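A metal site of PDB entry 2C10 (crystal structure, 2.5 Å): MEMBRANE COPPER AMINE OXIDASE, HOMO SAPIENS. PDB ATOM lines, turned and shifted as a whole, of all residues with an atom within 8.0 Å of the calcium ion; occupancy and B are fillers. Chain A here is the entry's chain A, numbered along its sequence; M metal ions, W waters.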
ATOM      1  N   LYS A  78      21.057 -11.019 -21.738  1.00  0.00           N
ATOM      2  CA  LYS A  78      20.306 -11.139 -20.504  1.00  0.00           C
ATOM      3  C   LYS A  78      18.797 -11.218 -20.751  1.00  0.00           C
ATOM      4  O   LYS A  78      18.122 -12.115 -20.205  1.00  0.00           O
ATOM      5  CB  LYS A  78      20.640  -9.985 -19.545  1.00  0.00           C
ATOM      6  CG  LYS A  78      19.865 -10.010 -18.234  1.00  0.00           C
ATOM      7  CD  LYS A  78      20.509  -9.101 -17.206  1.00  0.00           C
ATOM      8  CE  LYS A  78      19.835  -9.227 -15.870  1.00  0.00           C
ATOM      9  NZ  LYS A  78      20.267  -8.124 -14.983  1.00  0.00           N
ATOM     10  N   LEU A 331      18.487 -13.883  -6.370  1.00  0.00           N
ATOM     11  CA  LEU A 331      19.143 -12.738  -5.741  1.00  0.00           C
ATOM     12  C   LEU A 331      20.085 -12.037  -6.706  1.00  0.00           C
ATOM     13  O   LEU A 331      20.218 -10.824  -6.686  1.00  0.00           O
ATOM     14  CB  LEU A 331      19.930 -13.149  -4.504  1.00  0.00           C
ATOM     15  CG  LEU A 331      19.278 -13.988  -3.392  1.00  0.00           C
ATOM     16  CD1 LEU A 331      20.258 -14.196  -2.256  1.00  0.00           C
ATOM     17  CD2 LEU A 331      17.984 -13.349  -2.891  1.00  0.00           C
ATOM     18  N   VAL A 332      20.745 -12.804  -7.563  1.00  0.00           N
ATOM     19  CA  VAL A 332      21.813 -12.298  -8.420  1.00  0.00           C
ATOM     20  C   VAL A 332      21.759 -12.990  -9.784  1.00  0.00           C
ATOM     21  O   VAL A 332      21.698 -14.225  -9.862  1.00  0.00           O
ATOM     22  CB  VAL A 332      23.218 -12.587  -7.788  1.00  0.00           C
ATOM     23  CG1 VAL A 332      24.291 -11.934  -8.607  1.00  0.00           C
ATOM     24  CG2 VAL A 332      23.305 -12.132  -6.335  1.00  0.00           C
ATOM     25  N   TYR A 333      21.810 -12.189 -10.855  1.00  0.00           N
ATOM     26  CA  TYR A 333      21.886 -12.746 -12.205  1.00  0.00           C
ATOM     27  C   TYR A 333      23.311 -13.247 -12.533  1.00  0.00           C
ATOM     28  O   TYR A 333      23.471 -14.349 -13.058  1.00  0.00           O
ATOM     29  CB  TYR A 333      21.427 -11.720 -13.245  1.00  0.00           C
ATOM     30  CG  TYR A 333      21.616 -12.207 -14.665  1.00  0.00           C
ATOM     31  CD1 TYR A 333      20.612 -12.925 -15.335  1.00  0.00           C
ATOM     32  CD2 TYR A 333      22.816 -11.988 -15.345  1.00  0.00           C
ATOM     33  CE1 TYR A 333      20.799 -13.400 -16.648  1.00  0.00           C
ATOM     34  CE2 TYR A 333      23.002 -12.449 -16.649  1.00  0.00           C
ATOM     35  CZ  TYR A 333      21.989 -13.158 -17.291  1.00  0.00           C
ATOM     36  OH  TYR A 333      22.206 -13.599 -18.578  1.00  0.00           O
ATOM     37  N   GLU A 334      24.309 -12.424 -12.226  1.00  0.00           N
ATOM     38  CA  GLU A 334      25.710 -12.720 -12.484  1.00  0.00           C
ATOM     39  C   GLU A 334      26.600 -12.177 -11.347  1.00  0.00           C
ATOM     40  O   GLU A 334      26.421 -11.036 -10.927  1.00  0.00           O
ATOM     41  CB  GLU A 334      26.119 -12.098 -13.830  1.00  0.00           C
ATOM     42  CG  GLU A 334      27.627 -12.121 -14.139  1.00  0.00           C
ATOM     43  CD  GLU A 334      27.984 -11.511 -15.494  1.00  0.00           C
ATOM     44  OE1 GLU A 334      29.193 -11.351 -15.756  1.00  0.00           O
ATOM     45  OE2 GLU A 334      27.081 -11.185 -16.294  1.00  0.00           O
ATOM     46  N   VAL A 500      28.940  -7.453  -9.927  1.00  0.00           N
ATOM     47  CA  VAL A 500      27.868  -7.936  -9.065  1.00  0.00           C
ATOM     48  C   VAL A 500      26.504  -7.487  -9.576  1.00  0.00           C
ATOM     49  O   VAL A 500      26.012  -6.412  -9.221  1.00  0.00           O
ATOM     50  CB  VAL A 500      28.071  -7.460  -7.611  1.00  0.00           C
ATOM     51  CG1 VAL A 500      26.965  -7.971  -6.705  1.00  0.00           C
ATOM     52  CG2 VAL A 500      29.440  -7.911  -7.083  1.00  0.00           C
ATOM     53  N   ASP A 501      25.902  -8.328 -10.429  1.00  0.00           N
ATOM     54  CA  ASP A 501      24.593  -8.028 -10.988  1.00  0.00           C
ATOM     55  C   ASP A 501      23.486  -8.597 -10.108  1.00  0.00           C
ATOM     56  O   ASP A 501      22.936  -9.688 -10.358  1.00  0.00           O
ATOM     57  CB  ASP A 501      24.486  -8.544 -12.430  1.00  0.00           C
ATOM     58  CG  ASP A 501      23.222  -8.044 -13.152  1.00  0.00           C
ATOM     59  OD1 ASP A 501      22.460  -7.247 -12.564  1.00  0.00           O
ATOM     60  OD2 ASP A 501      23.000  -8.474 -14.322  1.00  0.00           O
ATOM     61  N   LEU A 502      23.190  -7.853  -9.038  1.00  0.00           N
ATOM     62  CA  LEU A 502      22.049  -8.098  -8.179  1.00  0.00           C
ATOM     63  C   LEU A 502      20.809  -7.694  -8.929  1.00  0.00           C
ATOM     64  O   LEU A 502      20.784  -6.634  -9.549  1.00  0.00           O
ATOM     65  CB  LEU A 502      22.150  -7.261  -6.895  1.00  0.00           C
ATOM     66  CG  LEU A 502      23.184  -7.656  -5.835  1.00  0.00           C
ATOM     67  CD1 LEU A 502      23.717  -6.423  -5.110  1.00  0.00           C
ATOM     68  CD2 LEU A 502      22.626  -8.706  -4.842  1.00  0.00           C
ATOM     69  N   ASP A 503      19.798  -8.563  -8.931  1.00  0.00           N
ATOM     70  CA  ASP A 503      18.469  -8.194  -9.393  1.00  0.00           C
ATOM     71  C   ASP A 503      17.546  -8.338  -8.197  1.00  0.00           C
ATOM     72  O   ASP A 503      16.871  -9.375  -8.054  1.00  0.00           O
ATOM     73  CB  ASP A 503      17.973  -9.133 -10.511  1.00  0.00           C
ATOM     74  CG  ASP A 503      18.692  -8.925 -11.831  1.00  0.00           C
ATOM     75  OD1 ASP A 503      19.396  -7.912 -12.000  1.00  0.00           O
ATOM     76  OD2 ASP A 503      18.497  -9.800 -12.721  1.00  0.00           O
ATOM     77  N   VAL A 504      17.533  -7.336  -7.312  1.00  0.00           N
ATOM     78  CA  VAL A 504      16.858  -7.483  -5.997  1.00  0.00           C
ATOM     79  C   VAL A 504      15.352  -7.538  -6.162  1.00  0.00           C
ATOM     80  O   VAL A 504      14.729  -6.514  -6.422  1.00  0.00           O
ATOM     81  CB  VAL A 504      17.247  -6.349  -4.998  1.00  0.00           C
ATOM     82  CG1 VAL A 504      16.561  -6.568  -3.654  1.00  0.00           C
ATOM     83  CG2 VAL A 504      18.761  -6.253  -4.824  1.00  0.00           C
ATOM     84  N   GLY A 506      13.625  -8.513  -8.603  1.00  0.00           N
ATOM     85  CA  GLY A 506      13.265  -7.962  -9.919  1.00  0.00           C
ATOM     86  C   GLY A 506      14.395  -7.123 -10.489  1.00  0.00           C
ATOM     87  O   GLY A 506      15.357  -6.795  -9.777  1.00  0.00           O
ATOM     88  N   LEU A 507      14.279  -6.758 -11.754  1.00  0.00           N
ATOM     89  CA  LEU A 507      15.312  -6.007 -12.471  1.00  0.00           C
ATOM     90  C   LEU A 507      15.458  -4.580 -11.968  1.00  0.00           C
ATOM     91  O   LEU A 507      16.572  -4.086 -11.804  1.00  0.00           O
ATOM     92  CB  LEU A 507      15.000  -5.919 -13.964  1.00  0.00           C
ATOM     93  CG  LEU A 507      15.153  -7.145 -14.850  1.00  0.00           C
ATOM     94  CD1 LEU A 507      14.082  -7.109 -15.932  1.00  0.00           C
ATOM     95  CD2 LEU A 507      16.561  -7.206 -15.450  1.00  0.00           C
ATOM     96  N   GLU A 508      14.332  -3.902 -11.763  1.00  0.00           N
ATOM     97  CA  GLU A 508      14.344  -2.467 -11.473  1.00  0.00           C
ATOM     98  C   GLU A 508      14.819  -2.256 -10.044  1.00  0.00           C
ATOM     99  O   GLU A 508      14.129  -2.629  -9.102  1.00  0.00           O
ATOM    100  CB  GLU A 508      12.953  -1.813 -11.674  1.00  0.00           C
ATOM    101  CG  GLU A 508      12.071  -2.426 -12.793  1.00  0.00           C
ATOM    102  CD  GLU A 508      12.713  -2.339 -14.168  1.00  0.00           C
ATOM    103  OE1 GLU A 508      13.508  -1.398 -14.396  1.00  0.00           O
ATOM    104  OE2 GLU A 508      12.431  -3.224 -15.030  1.00  0.00           O
ATOM    105  N   ASN A 509      16.014  -1.683  -9.902  1.00  0.00           N
ATOM    106  CA  ASN A 509      16.580  -1.393  -8.584  1.00  0.00           C
ATOM    107  C   ASN A 509      16.907   0.075  -8.332  1.00  0.00           C
ATOM    108  O   ASN A 509      17.042   0.888  -9.264  1.00  0.00           O
ATOM    109  CB  ASN A 509      17.796  -2.276  -8.303  1.00  0.00           C
ATOM    110  CG  ASN A 509      17.427  -3.737  -8.048  1.00  0.00           C
ATOM    111  OD1 ASN A 509      18.293  -4.619  -8.099  1.00  0.00           O
ATOM    112  ND2 ASN A 509      16.151  -3.989  -7.754  1.00  0.00           N
ATOM    113  N   LEU A 561      21.328  -2.067  -2.583  1.00  0.00           N
ATOM    114  CA  LEU A 561      20.393  -2.000  -3.712  1.00  0.00           C
ATOM    115  C   LEU A 561      19.090  -2.585  -3.255  1.00  0.00           C
ATOM    116  O   LEU A 561      19.078  -3.557  -2.505  1.00  0.00           O
ATOM    117  CB  LEU A 561      20.882  -2.763  -4.941  1.00  0.00           C
ATOM    118  CG  LEU A 561      22.231  -2.446  -5.576  1.00  0.00           C
ATOM    119  CD1 LEU A 561      22.204  -2.808  -7.053  1.00  0.00           C
ATOM    120  CD2 LEU A 561      22.635  -0.999  -5.415  1.00  0.00           C
ATOM    121  N   THR A 607      26.284   1.090 -11.750  1.00  0.00           N
ATOM    122  CA  THR A 607      25.954   1.601 -13.075  1.00  0.00           C
ATOM    123  C   THR A 607      24.726   0.862 -13.625  1.00  0.00           C
ATOM    124  O   THR A 607      24.342  -0.202 -13.109  1.00  0.00           O
ATOM    125  CB  THR A 607      27.130   1.379 -14.059  1.00  0.00           C
ATOM    126  OG1 THR A 607      27.384  -0.022 -14.211  1.00  0.00           O
ATOM    127  CG2 THR A 607      28.416   2.057 -13.568  1.00  0.00           C
ATOM    128  N   GLN A 608      24.101   1.413 -14.656  1.00  0.00           N
ATOM    129  CA  GLN A 608      23.117   0.663 -15.418  1.00  0.00           C
ATOM    130  C   GLN A 608      23.820  -0.521 -16.074  1.00  0.00           C
ATOM    131  O   GLN A 608      24.852  -0.353 -16.725  1.00  0.00           O
ATOM    132  CB  GLN A 608      22.478   1.547 -16.493  1.00  0.00           C
ATOM    133  CG  GLN A 608      21.675   2.724 -15.952  1.00  0.00           C
ATOM    134  CD  GLN A 608      20.929   3.501 -17.019  1.00  0.00           C
ATOM    135  OE1 GLN A 608      20.830   3.075 -18.181  1.00  0.00           O
ATOM    136  NE2 GLN A 608      20.385   4.659 -16.641  1.00  0.00           N
ATOM    137  N   ARG A 609      23.268  -1.719 -15.879  1.00  0.00           N
ATOM    138  CA  ARG A 609      23.733  -2.888 -16.614  1.00  0.00           C
ATOM    139  C   ARG A 609      23.318  -2.745 -18.077  1.00  0.00           C
ATOM    140  O   ARG A 609      22.138  -2.520 -18.388  1.00  0.00           O
ATOM    141  CB  ARG A 609      23.312  -4.202 -15.896  1.00  0.00           C
ATOM    142  CG  ARG A 609      22.638  -5.380 -16.665  1.00  0.00           C
ATOM    143  CD  ARG A 609      23.432  -5.897 -17.805  1.00  0.00           C
ATOM    144  NE  ARG A 609      23.648  -7.344 -17.792  1.00  0.00           N
ATOM    145  CZ  ARG A 609      23.470  -8.128 -18.858  1.00  0.00           C
ATOM    146  NH1 ARG A 609      23.739  -9.431 -18.773  1.00  0.00           N
ATOM    147  NH2 ARG A 609      23.037  -7.620 -19.996  1.00  0.00           N
ATOM    148  N   LYS A 644      16.226   1.090 -12.422  1.00  0.00           N
ATOM    149  CA  LYS A 644      16.820   0.575 -13.649  1.00  0.00           C
ATOM    150  C   LYS A 644      17.470  -0.758 -13.327  1.00  0.00           C
ATOM    151  O   LYS A 644      17.589  -1.113 -12.147  1.00  0.00           O
ATOM    152  CB  LYS A 644      17.869   1.559 -14.189  1.00  0.00           C
ATOM    153  CG  LYS A 644      17.277   2.797 -14.833  1.00  0.00           C
ATOM    154  CD  LYS A 644      16.814   2.493 -16.249  1.00  0.00           C
ATOM    155  CE  LYS A 644      16.057   3.671 -16.835  1.00  0.00           C
ATOM    156  NZ  LYS A 644      16.290   3.678 -18.300  1.00  0.00           N
ATOM    157  N   ASP A 645      17.887  -1.506 -14.352  1.00  0.00           N
ATOM    158  CA  ASP A 645      18.683  -2.705 -14.114  1.00  0.00           C
ATOM    159  C   ASP A 645      20.093  -2.280 -13.702  1.00  0.00           C
ATOM    160  O   ASP A 645      20.844  -1.724 -14.514  1.00  0.00           O
ATOM    161  CB  ASP A 645      18.721  -3.604 -15.342  1.00  0.00           C
ATOM    162  CG  ASP A 645      19.482  -4.895 -15.100  1.00  0.00           C
ATOM    163  OD1 ASP A 645      19.969  -5.085 -13.969  1.00  0.00           O
ATOM    164  OD2 ASP A 645      19.587  -5.724 -16.039  1.00  0.00           O
ATOM    165  N   LEU A 646      20.433  -2.516 -12.443  1.00  0.00           N
ATOM    166  CA  LEU A 646      21.704  -2.037 -11.891  1.00  0.00           C
ATOM    167  C   LEU A 646      22.725  -3.140 -11.763  1.00  0.00           C
ATOM    168  O   LEU A 646      22.375  -4.301 -11.524  1.00  0.00           O
ATOM    169  CB  LEU A 646      21.494  -1.430 -10.520  1.00  0.00           C
ATOM    170  CG  LEU A 646      20.551  -0.243 -10.391  1.00  0.00           C
ATOM    171  CD1 LEU A 646      20.743   0.352  -9.027  1.00  0.00           C
ATOM    172  CD2 LEU A 646      20.778   0.784 -11.469  1.00  0.00           C
ATOM    173  N   VAL A 647      23.993  -2.764 -11.926  1.00  0.00           N
ATOM    174  CA  VAL A 647      25.114  -3.641 -11.600  1.00  0.00           C
ATOM    175  C   VAL A 647      26.101  -2.867 -10.706  1.00  0.00           C
ATOM    176  O   VAL A 647      26.422  -1.703 -10.965  1.00  0.00           O
ATOM    177  CB  VAL A 647      25.823  -4.228 -12.882  1.00  0.00           C
ATOM    178  CG1 VAL A 647      26.139  -3.135 -13.912  1.00  0.00           C
ATOM    179  CG2 VAL A 647      27.088  -4.958 -12.533  1.00  0.00           C
ATOM    180  N   ALA A 648      26.565  -3.538  -9.652  1.00  0.00           N
ATOM    181  CA  ALA A 648      27.568  -2.978  -8.759  1.00  0.00           C
ATOM    182  C   ALA A 648      28.932  -3.518  -9.121  1.00  0.00           C
ATOM    183  O   ALA A 648      29.069  -4.696  -9.404  1.00  0.00           O
ATOM    184  CB  ALA A 648      27.227  -3.299  -7.311  1.00  0.00           C
HETATM  185 CA    CA M   1      20.674  -5.963 -11.766  1.00  0.00          CA
HETATM  186  O   HOH W   1      18.860  -4.578 -10.845  1.00  0.00           O
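OD2 of Asp 501 is in salt-bridge range of NZ of Lys 78, at 2.8 Å. The guanidinium group of Arg 609 lies within salt-bridge range of the side-chain carboxylate of Asp 501 (3.7 Å). The backbone NH of Tyr 333 lies within hydrogen-bond range of the backbone carbonyl oxygen of Asp 501 (2.8 Å). The backbone NH (N) of Asp 501 sits at hydrogen-bond distance from the backbone carbonyl oxygen (O) of Glu 334 (2.8 Å). NZ of Lys 78 is in salt-bridge range of OD2 of Asp 503 (3.3 Å). The backbone carbonyl oxygen of Leu 331 lies within hydrogen-bond range of the backbone NH of Asp 503. OD2 of Asp 645 is in salt-bridge range of NZ of Lys 78 (2.7 Å). O of Asp 645 lies within hydrogen-bond range of N of Arg 609, 2.8 Å away.
Merely in contact with the calcium ion: Lys 78. Six residues have an atom within 4 Å of the calcium ion: Lys 78, Asp 501, Leu 502, Asp 503, Asp 645 and Leu 646. The nearest printed residue that does not touch the calcium ion is Leu 507 (4.5 Å).
The calcium ion is bound by O of Leu 502 (2.3 Å), OD1 of Asp 501 (2.3 Å), OD1 of Asp 503 (2.3 Å), O of Leu 646 (2.4 Å), water W1 (2.5 Å) and OD1 of Asp 645 (2.5 Å).
Water W1 lies within hydrogen-bond range of the backbone carbonyl oxygen (O) of Leu 507 (2.5 Å), the side-chain amide oxygen (OD1) of Asn 509 (2.8 Å) and the backbone NH (N) of Leu 646 (3.0 Å).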
